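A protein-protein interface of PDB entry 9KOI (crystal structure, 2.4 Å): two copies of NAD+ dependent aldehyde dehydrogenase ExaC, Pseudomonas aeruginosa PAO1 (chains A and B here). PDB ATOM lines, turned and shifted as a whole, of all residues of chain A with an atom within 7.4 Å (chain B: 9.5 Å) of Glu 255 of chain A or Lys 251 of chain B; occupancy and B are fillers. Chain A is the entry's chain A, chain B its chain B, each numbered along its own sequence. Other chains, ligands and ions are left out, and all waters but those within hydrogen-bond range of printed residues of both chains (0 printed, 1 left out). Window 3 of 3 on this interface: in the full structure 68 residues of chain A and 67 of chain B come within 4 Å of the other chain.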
ATOM      1  N   ALA A 229     -11.783 -28.378   0.058  1.00  0.00           N
ATOM      2  CA  ALA A 229     -10.381 -28.103  -0.238  1.00  0.00           C
ATOM      3  C   ALA A 229      -9.509 -28.206   1.003  1.00  0.00           C
ATOM      4  O   ALA A 229      -8.305 -28.455   0.885  1.00  0.00           O
ATOM      5  CB  ALA A 229     -10.232 -26.716  -0.864  1.00  0.00           C
ATOM      6  N   THR A 230     -10.090 -28.013   2.184  1.00  0.00           N
ATOM      7  CA  THR A 230      -9.369 -28.088   3.446  1.00  0.00           C
ATOM      8  C   THR A 230      -9.630 -29.384   4.200  1.00  0.00           C
ATOM      9  O   THR A 230      -9.144 -29.536   5.324  1.00  0.00           O
ATOM     10  CB  THR A 230      -9.734 -26.895   4.333  1.00  0.00           C
ATOM     11  OG1 THR A 230     -11.160 -26.813   4.460  1.00  0.00           O
ATOM     12  CG2 THR A 230      -9.211 -25.604   3.727  1.00  0.00           C
ATOM     13  N   SER A 247      -3.381 -21.166  -6.507  1.00  0.00           N
ATOM     14  CA  SER A 247      -2.375 -21.020  -5.456  1.00  0.00           C
ATOM     15  C   SER A 247      -2.944 -21.346  -4.079  1.00  0.00           C
ATOM     16  O   SER A 247      -2.277 -21.988  -3.260  1.00  0.00           O
ATOM     17  CB  SER A 247      -1.803 -19.602  -5.474  1.00  0.00           C
ATOM     18  OG  SER A 247      -0.780 -19.455  -4.501  1.00  0.00           O
ATOM     19  N   HIS A 248      -4.180 -20.913  -3.807  1.00  0.00           N
ATOM     20  CA  HIS A 248      -4.811 -21.215  -2.526  1.00  0.00           C
ATOM     21  C   HIS A 248      -5.014 -22.715  -2.349  1.00  0.00           C
ATOM     22  O   HIS A 248      -4.759 -23.261  -1.270  1.00  0.00           O
ATOM     23  CB  HIS A 248      -6.142 -20.479  -2.410  1.00  0.00           C
ATOM     24  CG  HIS A 248      -6.889 -20.787  -1.150  1.00  0.00           C
ATOM     25  ND1 HIS A 248      -6.396 -20.487   0.101  1.00  0.00           N
ATOM     26  CD2 HIS A 248      -8.089 -21.383  -0.949  1.00  0.00           C
ATOM     27  CE1 HIS A 248      -7.263 -20.875   1.019  1.00  0.00           C
ATOM     28  NE2 HIS A 248      -8.298 -21.424   0.408  1.00  0.00           N
ATOM     29  N   ILE A 249      -5.510 -23.393  -3.389  1.00  0.00           N
ATOM     30  CA  ILE A 249      -5.615 -24.850  -3.337  1.00  0.00           C
ATOM     31  C   ILE A 249      -4.258 -25.451  -3.004  1.00  0.00           C
ATOM     32  O   ILE A 249      -4.144 -26.357  -2.172  1.00  0.00           O
ATOM     33  CB  ILE A 249      -6.169 -25.398  -4.666  1.00  0.00           C
ATOM     34  CG1 ILE A 249      -7.613 -24.942  -4.878  1.00  0.00           C
ATOM     35  CG2 ILE A 249      -6.075 -26.915  -4.698  1.00  0.00           C
ATOM     36  CD1 ILE A 249      -8.580 -25.493  -3.856  1.00  0.00           C
ATOM     37  N   LEU A 250      -3.205 -24.936  -3.643  1.00  0.00           N
ATOM     38  CA  LEU A 250      -1.856 -25.419  -3.375  1.00  0.00           C
ATOM     39  C   LEU A 250      -1.409 -25.075  -1.957  1.00  0.00           C
ATOM     40  O   LEU A 250      -0.596 -25.802  -1.376  1.00  0.00           O
ATOM     41  CB  LEU A 250      -0.884 -24.838  -4.404  1.00  0.00           C
ATOM     42  CG  LEU A 250      -1.054 -25.261  -5.867  1.00  0.00           C
ATOM     43  CD1 LEU A 250       0.003 -24.613  -6.750  1.00  0.00           C
ATOM     44  CD2 LEU A 250      -1.011 -26.765  -6.007  1.00  0.00           C
ATOM     45  N   LYS A 251      -1.909 -23.971  -1.390  1.00  0.00           N
ATOM     46  CA  LYS A 251      -1.649 -23.684   0.019  1.00  0.00           C
ATOM     47  C   LYS A 251      -2.370 -24.668   0.931  1.00  0.00           C
ATOM     48  O   LYS A 251      -1.758 -25.273   1.819  1.00  0.00           O
ATOM     49  CB  LYS A 251      -2.076 -22.259   0.367  1.00  0.00           C
ATOM     50  CG  LYS A 251      -0.966 -21.229   0.398  1.00  0.00           C
ATOM     51  CD  LYS A 251      -1.521 -19.889   0.857  1.00  0.00           C
ATOM     52  CE  LYS A 251      -0.430 -18.842   0.994  1.00  0.00           C
ATOM     53  NZ  LYS A 251      -0.007 -18.674   2.417  1.00  0.00           N
ATOM     54  N   CYS A 252      -3.681 -24.836   0.729  1.00  0.00           N
ATOM     55  CA  CYS A 252      -4.445 -25.794   1.524  1.00  0.00           C
ATOM     56  C   CYS A 252      -3.905 -27.207   1.356  1.00  0.00           C
ATOM     57  O   CYS A 252      -3.876 -27.986   2.316  1.00  0.00           O
ATOM     58  CB  CYS A 252      -5.924 -25.723   1.156  1.00  0.00           C
ATOM     59  SG  CYS A 252      -6.699 -24.153   1.601  1.00  0.00           S
ATOM     60  N   ALA A 253      -3.474 -27.561   0.141  1.00  0.00           N
ATOM     61  CA  ALA A 253      -2.852 -28.865  -0.054  1.00  0.00           C
ATOM     62  C   ALA A 253      -1.534 -28.945   0.703  1.00  0.00           C
ATOM     63  O   ALA A 253      -1.193 -29.995   1.258  1.00  0.00           O
ATOM     64  CB  ALA A 253      -2.641 -29.131  -1.544  1.00  0.00           C
ATOM     65  N   ALA A 254      -0.780 -27.844   0.724  1.00  0.00           N
ATOM     66  CA  ALA A 254       0.449 -27.789   1.507  1.00  0.00           C
ATOM     67  C   ALA A 254       0.175 -28.008   2.988  1.00  0.00           C
ATOM     68  O   ALA A 254       1.002 -28.602   3.691  1.00  0.00           O
ATOM     69  CB  ALA A 254       1.159 -26.456   1.284  1.00  0.00           C
ATOM     70  N   GLU A 255      -0.970 -27.522   3.482  1.00  0.00           N
ATOM     71  CA  GLU A 255      -1.267 -27.617   4.910  1.00  0.00           C
ATOM     72  C   GLU A 255      -1.314 -29.067   5.369  1.00  0.00           C
ATOM     73  O   GLU A 255      -0.962 -29.368   6.515  1.00  0.00           O
ATOM     74  CB  GLU A 255      -2.618 -26.956   5.210  1.00  0.00           C
ATOM     75  CG  GLU A 255      -2.769 -25.491   4.814  1.00  0.00           C
ATOM     76  CD  GLU A 255      -2.046 -24.530   5.735  1.00  0.00           C
ATOM     77  OE1 GLU A 255      -1.474 -24.979   6.749  1.00  0.00           O
ATOM     78  OE2 GLU A 255      -2.068 -23.314   5.445  1.00  0.00           O
ATOM     79  N   ASN A 256      -1.736 -29.972   4.489  1.00  0.00           N
ATOM     80  CA  ASN A 256      -1.941 -31.372   4.826  1.00  0.00           C
ATOM     81  C   ASN A 256      -0.989 -32.307   4.092  1.00  0.00           C
ATOM     82  O   ASN A 256      -1.106 -33.529   4.246  1.00  0.00           O
ATOM     83  CB  ASN A 256      -3.392 -31.775   4.538  1.00  0.00           C
ATOM     84  CG  ASN A 256      -4.396 -30.967   5.346  1.00  0.00           C
ATOM     85  OD1 ASN A 256      -4.023 -30.056   6.090  1.00  0.00           O
ATOM     86  ND2 ASN A 256      -5.673 -31.290   5.196  1.00  0.00           N
ATOM     87  N   ILE A 257      -0.057 -31.769   3.302  1.00  0.00           N
ATOM     88  CA  ILE A 257       0.954 -32.550   2.593  1.00  0.00           C
ATOM     89  C   ILE A 257       0.290 -33.616   1.730  1.00  0.00           C
ATOM     90  O   ILE A 257       0.508 -34.819   1.922  1.00  0.00           O
ATOM     91  CB  ILE A 257       1.968 -33.170   3.572  1.00  0.00           C
ATOM     92  CG1 ILE A 257       2.346 -32.152   4.650  1.00  0.00           C
ATOM     93  CG2 ILE A 257       3.220 -33.630   2.834  1.00  0.00           C
ATOM     94  CD1 ILE A 257       3.435 -32.621   5.580  1.00  0.00           C
ATOM     95  N   ILE A 258      -0.545 -33.183   0.790  1.00  0.00           N
ATOM     96  CA  ILE A 258      -1.180 -34.093  -0.161  1.00  0.00           C
ATOM     97  C   ILE A 258      -0.759 -33.683  -1.566  1.00  0.00           C
ATOM     98  O   ILE A 258      -0.511 -32.493  -1.814  1.00  0.00           O
ATOM     99  CB  ILE A 258      -2.710 -34.089  -0.006  1.00  0.00           C
ATOM    100  CG1 ILE A 258      -3.294 -32.731  -0.405  1.00  0.00           C
ATOM    101  CG2 ILE A 258      -3.104 -34.438   1.422  1.00  0.00           C
ATOM    102  CD1 ILE A 258      -4.806 -32.711  -0.491  1.00  0.00           C
ATOM    103  N   GLU B 226      15.774 -19.977   3.207  1.00  0.00           N
ATOM    104  CA  GLU B 226      14.583 -19.163   2.980  1.00  0.00           C
ATOM    105  C   GLU B 226      14.683 -18.404   1.663  1.00  0.00           C
ATOM    106  O   GLU B 226      13.757 -18.434   0.845  1.00  0.00           O
ATOM    107  CB  GLU B 226      14.362 -18.197   4.142  1.00  0.00           C
ATOM    108  CG  GLU B 226      13.127 -17.328   3.966  1.00  0.00           C
ATOM    109  CD  GLU B 226      11.839 -18.130   3.993  1.00  0.00           C
ATOM    110  OE1 GLU B 226      11.835 -19.240   4.569  1.00  0.00           O
ATOM    111  OE2 GLU B 226      10.831 -17.660   3.427  1.00  0.00           O
ATOM    112  N   ALA B 229      14.034 -20.954  -1.044  1.00  0.00           N
ATOM    113  CA  ALA B 229      12.699 -21.539  -1.139  1.00  0.00           C
ATOM    114  C   ALA B 229      11.668 -20.564  -1.701  1.00  0.00           C
ATOM    115  O   ALA B 229      10.677 -20.998  -2.299  1.00  0.00           O
ATOM    116  CB  ALA B 229      12.249 -22.040   0.233  1.00  0.00           C
ATOM    117  N   THR B 230      11.878 -19.261  -1.531  1.00  0.00           N
ATOM    118  CA  THR B 230      10.939 -18.259  -2.017  1.00  0.00           C
ATOM    119  C   THR B 230      11.409 -17.585  -3.296  1.00  0.00           C
ATOM    120  O   THR B 230      10.738 -16.668  -3.778  1.00  0.00           O
ATOM    121  CB  THR B 230      10.683 -17.194  -0.946  1.00  0.00           C
ATOM    122  OG1 THR B 230      11.930 -16.625  -0.525  1.00  0.00           O
ATOM    123  CG2 THR B 230       9.975 -17.801   0.253  1.00  0.00           C
ATOM    124  N   ILE B 237      11.218 -26.449  -6.679  1.00  0.00           N
ATOM    125  CA  ILE B 237      11.923 -26.614  -5.416  1.00  0.00           C
ATOM    126  C   ILE B 237      11.902 -28.085  -5.021  1.00  0.00           C
ATOM    127  O   ILE B 237      10.943 -28.814  -5.302  1.00  0.00           O
ATOM    128  CB  ILE B 237      11.325 -25.721  -4.304  1.00  0.00           C
ATOM    129  CG1 ILE B 237      12.268 -25.661  -3.099  1.00  0.00           C
ATOM    130  CG2 ILE B 237       9.939 -26.200  -3.896  1.00  0.00           C
ATOM    131  CD1 ILE B 237      13.602 -25.009  -3.405  1.00  0.00           C
ATOM    132  N   THR B 243       9.244 -32.546   8.691  1.00  0.00           N
ATOM    133  CA  THR B 243       7.887 -32.223   8.254  1.00  0.00           C
ATOM    134  C   THR B 243       7.496 -30.751   8.391  1.00  0.00           C
ATOM    135  O   THR B 243       6.897 -30.218   7.441  1.00  0.00           O
ATOM    136  CB  THR B 243       6.899 -33.122   9.016  1.00  0.00           C
ATOM    137  OG1 THR B 243       7.182 -34.496   8.728  1.00  0.00           O
ATOM    138  CG2 THR B 243       5.467 -32.819   8.617  1.00  0.00           C
ATOM    139  N   PRO B 244       7.772 -30.047   9.501  1.00  0.00           N
ATOM    140  CA  PRO B 244       7.353 -28.633   9.568  1.00  0.00           C
ATOM    141  C   PRO B 244       7.989 -27.747   8.506  1.00  0.00           C
ATOM    142  O   PRO B 244       7.311 -26.864   7.964  1.00  0.00           O
ATOM    143  CB  PRO B 244       7.780 -28.212  10.982  1.00  0.00           C
ATOM    144  CG  PRO B 244       7.809 -29.477  11.754  1.00  0.00           C
ATOM    145  CD  PRO B 244       8.326 -30.500  10.789  1.00  0.00           C
ATOM    146  N   VAL B 245       9.271 -27.949   8.190  1.00  0.00           N
ATOM    147  CA  VAL B 245       9.896 -27.136   7.154  1.00  0.00           C
ATOM    148  C   VAL B 245       9.420 -27.563   5.774  1.00  0.00           C
ATOM    149  O   VAL B 245       9.285 -26.725   4.869  1.00  0.00           O
ATOM    150  CB  VAL B 245      11.428 -27.204   7.269  1.00  0.00           C
ATOM    151  CG1 VAL B 245      12.067 -25.995   6.597  1.00  0.00           C
ATOM    152  CG2 VAL B 245      11.844 -27.291   8.729  1.00  0.00           C
ATOM    153  N   GLY B 246       9.149 -28.857   5.587  1.00  0.00           N
ATOM    154  CA  GLY B 246       8.585 -29.316   4.327  1.00  0.00           C
ATOM    155  C   GLY B 246       7.233 -28.693   4.044  1.00  0.00           C
ATOM    156  O   GLY B 246       6.995 -28.157   2.960  1.00  0.00           O
ATOM    157  N   SER B 247       6.318 -28.788   5.017  1.00  0.00           N
ATOM    158  CA  SER B 247       5.029 -28.112   4.917  1.00  0.00           C
ATOM    159  C   SER B 247       5.205 -26.661   4.490  1.00  0.00           C
ATOM    160  O   SER B 247       4.430 -26.144   3.678  1.00  0.00           O
ATOM    161  CB  SER B 247       4.295 -28.200   6.257  1.00  0.00           C
ATOM    162  OG  SER B 247       3.003 -27.623   6.184  1.00  0.00           O
ATOM    163  N   HIS B 248       6.217 -25.985   5.041  1.00  0.00           N
ATOM    164  CA  HIS B 248       6.531 -24.624   4.617  1.00  0.00           C
ATOM    165  C   HIS B 248       7.032 -24.582   3.176  1.00  0.00           C
ATOM    166  O   HIS B 248       6.626 -23.708   2.400  1.00  0.00           O
ATOM    167  CB  HIS B 248       7.563 -24.007   5.558  1.00  0.00           C
ATOM    168  CG  HIS B 248       7.928 -22.599   5.208  1.00  0.00           C
ATOM    169  ND1 HIS B 248       7.044 -21.549   5.329  1.00  0.00           N
ATOM    170  CD2 HIS B 248       9.079 -22.069   4.732  1.00  0.00           C
ATOM    171  CE1 HIS B 248       7.636 -20.431   4.946  1.00  0.00           C
ATOM    172  NE2 HIS B 248       8.871 -20.720   4.578  1.00  0.00           N
ATOM    173  N   ILE B 249       7.934 -25.501   2.806  1.00  0.00           N
ATOM    174  CA  ILE B 249       8.442 -25.561   1.433  1.00  0.00           C
ATOM    175  C   ILE B 249       7.295 -25.655   0.435  1.00  0.00           C
ATOM    176  O   ILE B 249       7.285 -24.963  -0.591  1.00  0.00           O
ATOM    177  CB  ILE B 249       9.421 -26.740   1.272  1.00  0.00           C
ATOM    178  CG1 ILE B 249      10.683 -26.527   2.111  1.00  0.00           C
ATOM    179  CG2 ILE B 249       9.796 -26.928  -0.193  1.00  0.00           C
ATOM    180  CD1 ILE B 249      11.512 -25.341   1.686  1.00  0.00           C
ATOM    181  N   LEU B 250       6.308 -26.506   0.725  1.00  0.00           N
ATOM    182  CA  LEU B 250       5.167 -26.655  -0.171  1.00  0.00           C
ATOM    183  C   LEU B 250       4.339 -25.380  -0.239  1.00  0.00           C
ATOM    184  O   LEU B 250       3.743 -25.079  -1.279  1.00  0.00           O
ATOM    185  CB  LEU B 250       4.301 -27.825   0.293  1.00  0.00           C
ATOM    186  CG  LEU B 250       4.808 -29.232  -0.024  1.00  0.00           C
ATOM    187  CD1 LEU B 250       3.952 -30.272   0.673  1.00  0.00           C
ATOM    188  CD2 LEU B 250       4.809 -29.468  -1.517  1.00  0.00           C
ATOM    189  N   LYS B 251       4.297 -24.621   0.856  1.00  0.00           N
ATOM    190  CA  LYS B 251       3.678 -23.301   0.831  1.00  0.00           C
ATOM    191  C   LYS B 251       4.494 -22.332  -0.016  1.00  0.00           C
ATOM    192  O   LYS B 251       3.931 -21.568  -0.810  1.00  0.00           O
ATOM    193  CB  LYS B 251       3.485 -22.792   2.259  1.00  0.00           C
ATOM    194  CG  LYS B 251       2.521 -23.670   3.044  1.00  0.00           C
ATOM    195  CD  LYS B 251       2.608 -23.490   4.546  1.00  0.00           C
ATOM    196  CE  LYS B 251       1.776 -24.563   5.239  1.00  0.00           C
ATOM    197  NZ  LYS B 251       1.889 -24.522   6.721  1.00  0.00           N
ATOM    198  N   CYS B 252       5.819 -22.332   0.157  1.00  0.00           N
ATOM    199  CA  CYS B 252       6.673 -21.498  -0.683  1.00  0.00           C
ATOM    200  C   CYS B 252       6.477 -21.825  -2.159  1.00  0.00           C
ATOM    201  O   CYS B 252       6.468 -20.926  -3.007  1.00  0.00           O
ATOM    202  CB  CYS B 252       8.139 -21.690  -0.293  1.00  0.00           C
ATOM    203  SG  CYS B 252       8.530 -21.302   1.425  1.00  0.00           S
ATOM    204  N   ALA B 253       6.321 -23.109  -2.482  1.00  0.00           N
ATOM    205  CA  ALA B 253       6.043 -23.507  -3.858  1.00  0.00           C
ATOM    206  C   ALA B 253       4.644 -23.084  -4.294  1.00  0.00           C
ATOM    207  O   ALA B 253       4.441 -22.703  -5.453  1.00  0.00           O
ATOM    208  CB  ALA B 253       6.214 -25.018  -4.009  1.00  0.00           C
ATOM    209  N   ALA B 254       3.669 -23.157  -3.384  1.00  0.00           N
ATOM    210  CA  ALA B 254       2.294 -22.795  -3.719  1.00  0.00           C
ATOM    211  C   ALA B 254       2.175 -21.347  -4.183  1.00  0.00           C
ATOM    212  O   ALA B 254       1.408 -21.047  -5.105  1.00  0.00           O
ATOM    213  CB  ALA B 254       1.391 -23.034  -2.510  1.00  0.00           C
ATOM    214  N   GLU B 255       2.922 -20.434  -3.555  1.00  0.00           N
ATOM    215  CA  GLU B 255       2.778 -19.015  -3.868  1.00  0.00           C
ATOM    216  C   GLU B 255       3.152 -18.703  -5.312  1.00  0.00           C
ATOM    217  O   GLU B 255       2.626 -17.747  -5.894  1.00  0.00           O
ATOM    218  CB  GLU B 255       3.617 -18.171  -2.908  1.00  0.00           C
ATOM    219  CG  GLU B 255       2.819 -17.575  -1.754  1.00  0.00           C
ATOM    220  CD  GLU B 255       1.673 -16.696  -2.225  1.00  0.00           C
ATOM    221  OE1 GLU B 255       1.939 -15.602  -2.766  1.00  0.00           O
ATOM    222  OE2 GLU B 255       0.503 -17.097  -2.049  1.00  0.00           O
ATOM    223  N   ASN B 256       4.048 -19.489  -5.907  1.00  0.00           N
ATOM    224  CA  ASN B 256       4.571 -19.199  -7.233  1.00  0.00           C
ATOM    225  C   ASN B 256       4.140 -20.212  -8.286  1.00  0.00           C
ATOM    226  O   ASN B 256       4.557 -20.089  -9.443  1.00  0.00           O
ATOM    227  CB  ASN B 256       6.102 -19.123  -7.181  1.00  0.00           C
ATOM    228  CG  ASN B 256       6.600 -18.184  -6.098  1.00  0.00           C
ATOM    229  OD1 ASN B 256       5.888 -17.270  -5.680  1.00  0.00           O
ATOM    230  ND2 ASN B 256       7.824 -18.407  -5.634  1.00  0.00           N
ATOM    231  N   ILE B 257       3.312 -21.192  -7.918  1.00  0.00           N
ATOM    232  CA  ILE B 257       2.766 -22.192  -8.833  1.00  0.00           C
ATOM    233  C   ILE B 257       3.944 -22.843  -9.556  1.00  0.00           C
ATOM    234  O   ILE B 257       4.072 -22.776 -10.783  1.00  0.00           O
ATOM    235  CB  ILE B 257       1.725 -21.558  -9.782  1.00  0.00           C
ATOM    236  CG1 ILE B 257       0.499 -21.146  -8.971  1.00  0.00           C
ATOM    237  CG2 ILE B 257       1.204 -22.555 -10.816  1.00  0.00           C
ATOM    238  CD1 ILE B 257      -0.224 -19.943  -9.516  1.00  0.00           C
ATOM    239  N   ILE B 258       4.851 -23.419  -8.775  1.00  0.00           N
ATOM    240  CA  ILE B 258       5.996 -24.155  -9.300  1.00  0.00           C
ATOM    241  C   ILE B 258       5.938 -25.576  -8.755  1.00  0.00           C
ATOM    242  O   ILE B 258       5.430 -25.790  -7.644  1.00  0.00           O
ATOM    243  CB  ILE B 258       7.321 -23.463  -8.940  1.00  0.00           C
ATOM    244  CG1 ILE B 258       7.388 -23.192  -7.436  1.00  0.00           C
ATOM    245  CG2 ILE B 258       7.480 -22.174  -9.735  1.00  0.00           C
ATOM    246  CD1 ILE B 258       8.716 -22.640  -6.974  1.00  0.00           C
ATOM    247  N   SER B 260       6.984 -28.996  -6.866  1.00  0.00           N
ATOM    248  CA  SER B 260       7.705 -29.240  -5.629  1.00  0.00           C
ATOM    249  C   SER B 260       7.727 -30.735  -5.355  1.00  0.00           C
ATOM    250  O   SER B 260       6.726 -31.428  -5.565  1.00  0.00           O
ATOM    251  CB  SER B 260       7.063 -28.496  -4.455  1.00  0.00           C
ATOM    252  OG  SER B 260       5.677 -28.772  -4.393  1.00  0.00           O
ATOM    253  N   VAL B 262       8.951 -33.076  -1.985  1.00  0.00           N
ATOM    254  CA  VAL B 262       9.388 -33.014  -0.597  1.00  0.00           C
ATOM    255  C   VAL B 262       9.399 -34.425  -0.036  1.00  0.00           C
ATOM    256  O   VAL B 262       8.396 -35.143  -0.125  1.00  0.00           O
ATOM    257  CB  VAL B 262       8.483 -32.100   0.249  1.00  0.00           C
ATOM    258  CG1 VAL B 262       8.896 -30.648   0.087  1.00  0.00           C
ATOM    259  CG2 VAL B 262       7.023 -32.290  -0.139  1.00  0.00           C
ATOM    260  N   LEU B 264      10.028 -36.315   3.553  1.00  0.00           N
ATOM    261  CA  LEU B 264      10.022 -35.872   4.938  1.00  0.00           C
ATOM    262  C   LEU B 264      10.359 -37.009   5.892  1.00  0.00           C
ATOM    263  O   LEU B 264      11.133 -37.908   5.548  1.00  0.00           O
ATOM    264  CB  LEU B 264       8.660 -35.269   5.288  1.00  0.00           C
ATOM    265  CG  LEU B 264       8.196 -34.158   4.345  1.00  0.00           C
ATOM    266  CD1 LEU B 264       6.781 -33.726   4.680  1.00  0.00           C
ATOM    267  CD2 LEU B 264       9.148 -32.971   4.389  1.00  0.00           C
ATOM    268  N   GLU B 428       1.030 -41.046  11.547  1.00  0.00           N
ATOM    269  CA  GLU B 428       0.794 -40.053  10.509  1.00  0.00           C
ATOM    270  C   GLU B 428       1.789 -40.162   9.363  1.00  0.00           C
ATOM    271  O   GLU B 428       1.618 -39.477   8.350  1.00  0.00           O
ATOM    272  CB  GLU B 428       0.814 -38.636  11.092  1.00  0.00           C
ATOM    273  CG  GLU B 428       2.035 -38.279  11.912  1.00  0.00           C
ATOM    274  CD  GLU B 428       2.128 -36.786  12.169  1.00  0.00           C
ATOM    275  OE1 GLU B 428       1.136 -36.205  12.658  1.00  0.00           O
ATOM    276  OE2 GLU B 428       3.188 -36.193  11.876  1.00  0.00           O
ATOM    277  N   LYS B 473       0.922 -40.241   3.051  1.00  0.00           N
ATOM    278  CA  LYS B 473       0.501 -39.359   4.140  1.00  0.00           C
ATOM    279  C   LYS B 473       1.450 -38.180   4.322  1.00  0.00           C
ATOM    280  O   LYS B 473       1.857 -37.546   3.346  1.00  0.00           O
ATOM    281  CB  LYS B 473       0.389 -40.157   5.444  1.00  0.00           C
ATOM    282  CG  LYS B 473      -0.677 -41.251   5.427  1.00  0.00           C
ATOM    283  CD  LYS B 473      -0.394 -42.309   6.488  1.00  0.00           C
ATOM    284  CE  LYS B 473      -1.630 -42.674   7.304  1.00  0.00           C
ATOM    285  NZ  LYS B 473      -1.622 -44.120   7.682  1.00  0.00           N
ATOM    286  N   LYS B 474       1.813 -37.884   5.570  1.00  0.00           N
ATOM    287  CA  LYS B 474       2.756 -36.810   5.863  1.00  0.00           C
ATOM    288  C   LYS B 474       4.209 -37.193   5.625  1.00  0.00           C
ATOM    289  O   LYS B 474       5.097 -36.461   6.073  1.00  0.00           O
ATOM    290  CB  LYS B 474       2.605 -36.326   7.305  1.00  0.00           C
ATOM    291  CG  LYS B 474       1.384 -35.472   7.571  1.00  0.00           C
ATOM    292  CD  LYS B 474       1.059 -35.463   9.055  1.00  0.00           C
ATOM    293  CE  LYS B 474       0.383 -34.166   9.475  1.00  0.00           C
ATOM    294  NZ  LYS B 474       1.290 -33.287  10.267  1.00  0.00           N
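Of the 26 printed residues of chain B, 8 touch a printed residue of chain A. Printed residues of chain B that touch a printed residue of chain A: Thr 243, Ser 247, Leu 250, Lys 251, Ala 254, Glu 255, Leu 264 and Lys 473. Hydrophobic or aromatic side chains of chain B within 4 Å of the printed part of chain A: Leu 250, Ala 254 and Leu 264. Printed residues of chain A that touch a printed residue of chain B: Ser 247, Leu 250, Lys 251, Ala 254, Glu 255 and Ile 257. Among the printed residues, 12 pairs touch across the chains. Among the printed residues, Asp or Glu carboxylates within 4 Å of a Lys or Arg side-chain nitrogen of the other chain: Glu 255 of chain A with Lys 251 of chain B (3.4 Å).
Ser 247 of chain A touches Glu 255 of chain B (OG to OE2, 3.6 Å). Leu 250 of chain A touches Ala 254 of chain B. Lys 251 of chain A touches Ala 254 of chain B (N to CB, 3.6 Å). CE of Lys 251 of chain A touches OE2 of Glu 255 of chain B, 3.6 Å away. Ala 254 of chain A touches Leu 250 of chain B (CB to CB, 3.6 Å). Ala 254 of chain A touches Lys 251 of chain B (CB to CG, 3.6 Å). CD1 of Ile 257 of chain A touches CG2 of Thr 243 of chain B, 3.7 Å away. Ile 257 of chain A touches Leu 264 of chain B (CD1 to CD1, 3.6 Å).
Ser 247 of chain A touches Glu 255 of chain B, but with the chains exchanged Glu 255 of chain A does not touch Ser 247 of chain B (4.3 Å). Leu 250 of chain A touches Ala 254 of chain B, and with the chains exchanged Ala 254 of chain A touches Leu 250 of chain B. Lys 251 of chain A touches Ala 254 of chain B, and with the chains exchanged Ala 254 of chain A touches Lys 251 of chain B. Lys 251 of chain A touches Glu 255 of chain B, and with the chains exchanged Glu 255 of chain A touches Lys 251 of chain B. Positions printed for both chains: 229, 230, 247, 248, 249, 250, 251, 252, 253, 254, 255, 256, 257 and 258. Of the 12 pairs that touch across the chains among the printed residues, 8 have their exchanged pair printed and touching as well.
The backbone carbonyl oxygen of Ala 254 of chain B lies within hydrogen-bond range of the side-chain hydroxyl of Ser 247 of chain A, 2.8 Å away. The side-chain hydroxyl (OG) of Ser 247 of chain B lies within hydrogen-bond range of the backbone carbonyl oxygen (O) of Ala 254 of chain A. The side-chain amino group (NZ) of Lys 251 of chain B is in salt-bridge range of the side-chain carboxylate (OE1) of Glu 255 of chain A, 3.4 Å away. The backbone carbonyl oxygen (O) of Ile 257 of chain A sits close to the backbone carbonyl oxygen (O) of Lys 473 of chain B, at 3.4 Å.
The side-chain hydroxyl of Ser 247 of chain B lies within hydrogen-bond range of the side-chain amino group of Lys 251 of chain B (3.3 Å).
Glu 255 of chain A touches just one residue of chain B: Lys 251 (3.4 Å). Of chain A, only Ala 254 and Glu 255 come within 4 Å of Lys 251 of chain B. No residue of chain B comes within 4 Å of Cys 252 of chain A. Of the printed residues of chain B, Ala 254 of chain A touches Ser 247 (3.3 Å), Leu 250 (3.6 Å) and Lys 251 (3.6 Å). No residue of chain B comes within 4 Å of Asn 256 of chain A. Of the printed residues of chain A, Leu 264 of chain B touches Ile 257. Printed residues of chain A within 4 Å of Ala 254 of chain B: Ser 247, Leu 250 and Lys 251. Printed residues of chain A within 4 Å of Glu 255 of chain B: Ser 247 (3.6 Å) and Lys 251 (3.6 Å). Of the printed residues of chain B, Ile 257 of chain A touches Thr 243 (3.7 Å), Leu 264 (3.6 Å) and Lys 473 (3.4 Å). Of the printed residues of chain A, Leu 250 of chain B touches Ala 254 (3.6 Å). His 248 of chain A touches none of the printed residues of chain B. Ala 229 of chain B touches none of the printed residues of chain A. The nearest residue of chain A that does not touch Lys 251 of chain B is Lys 251 of chain A (4.7 Å). The nearest printed residue of chain A that does not touch Leu 250 of chain B is Ile 257 of chain A (4.1 Å).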
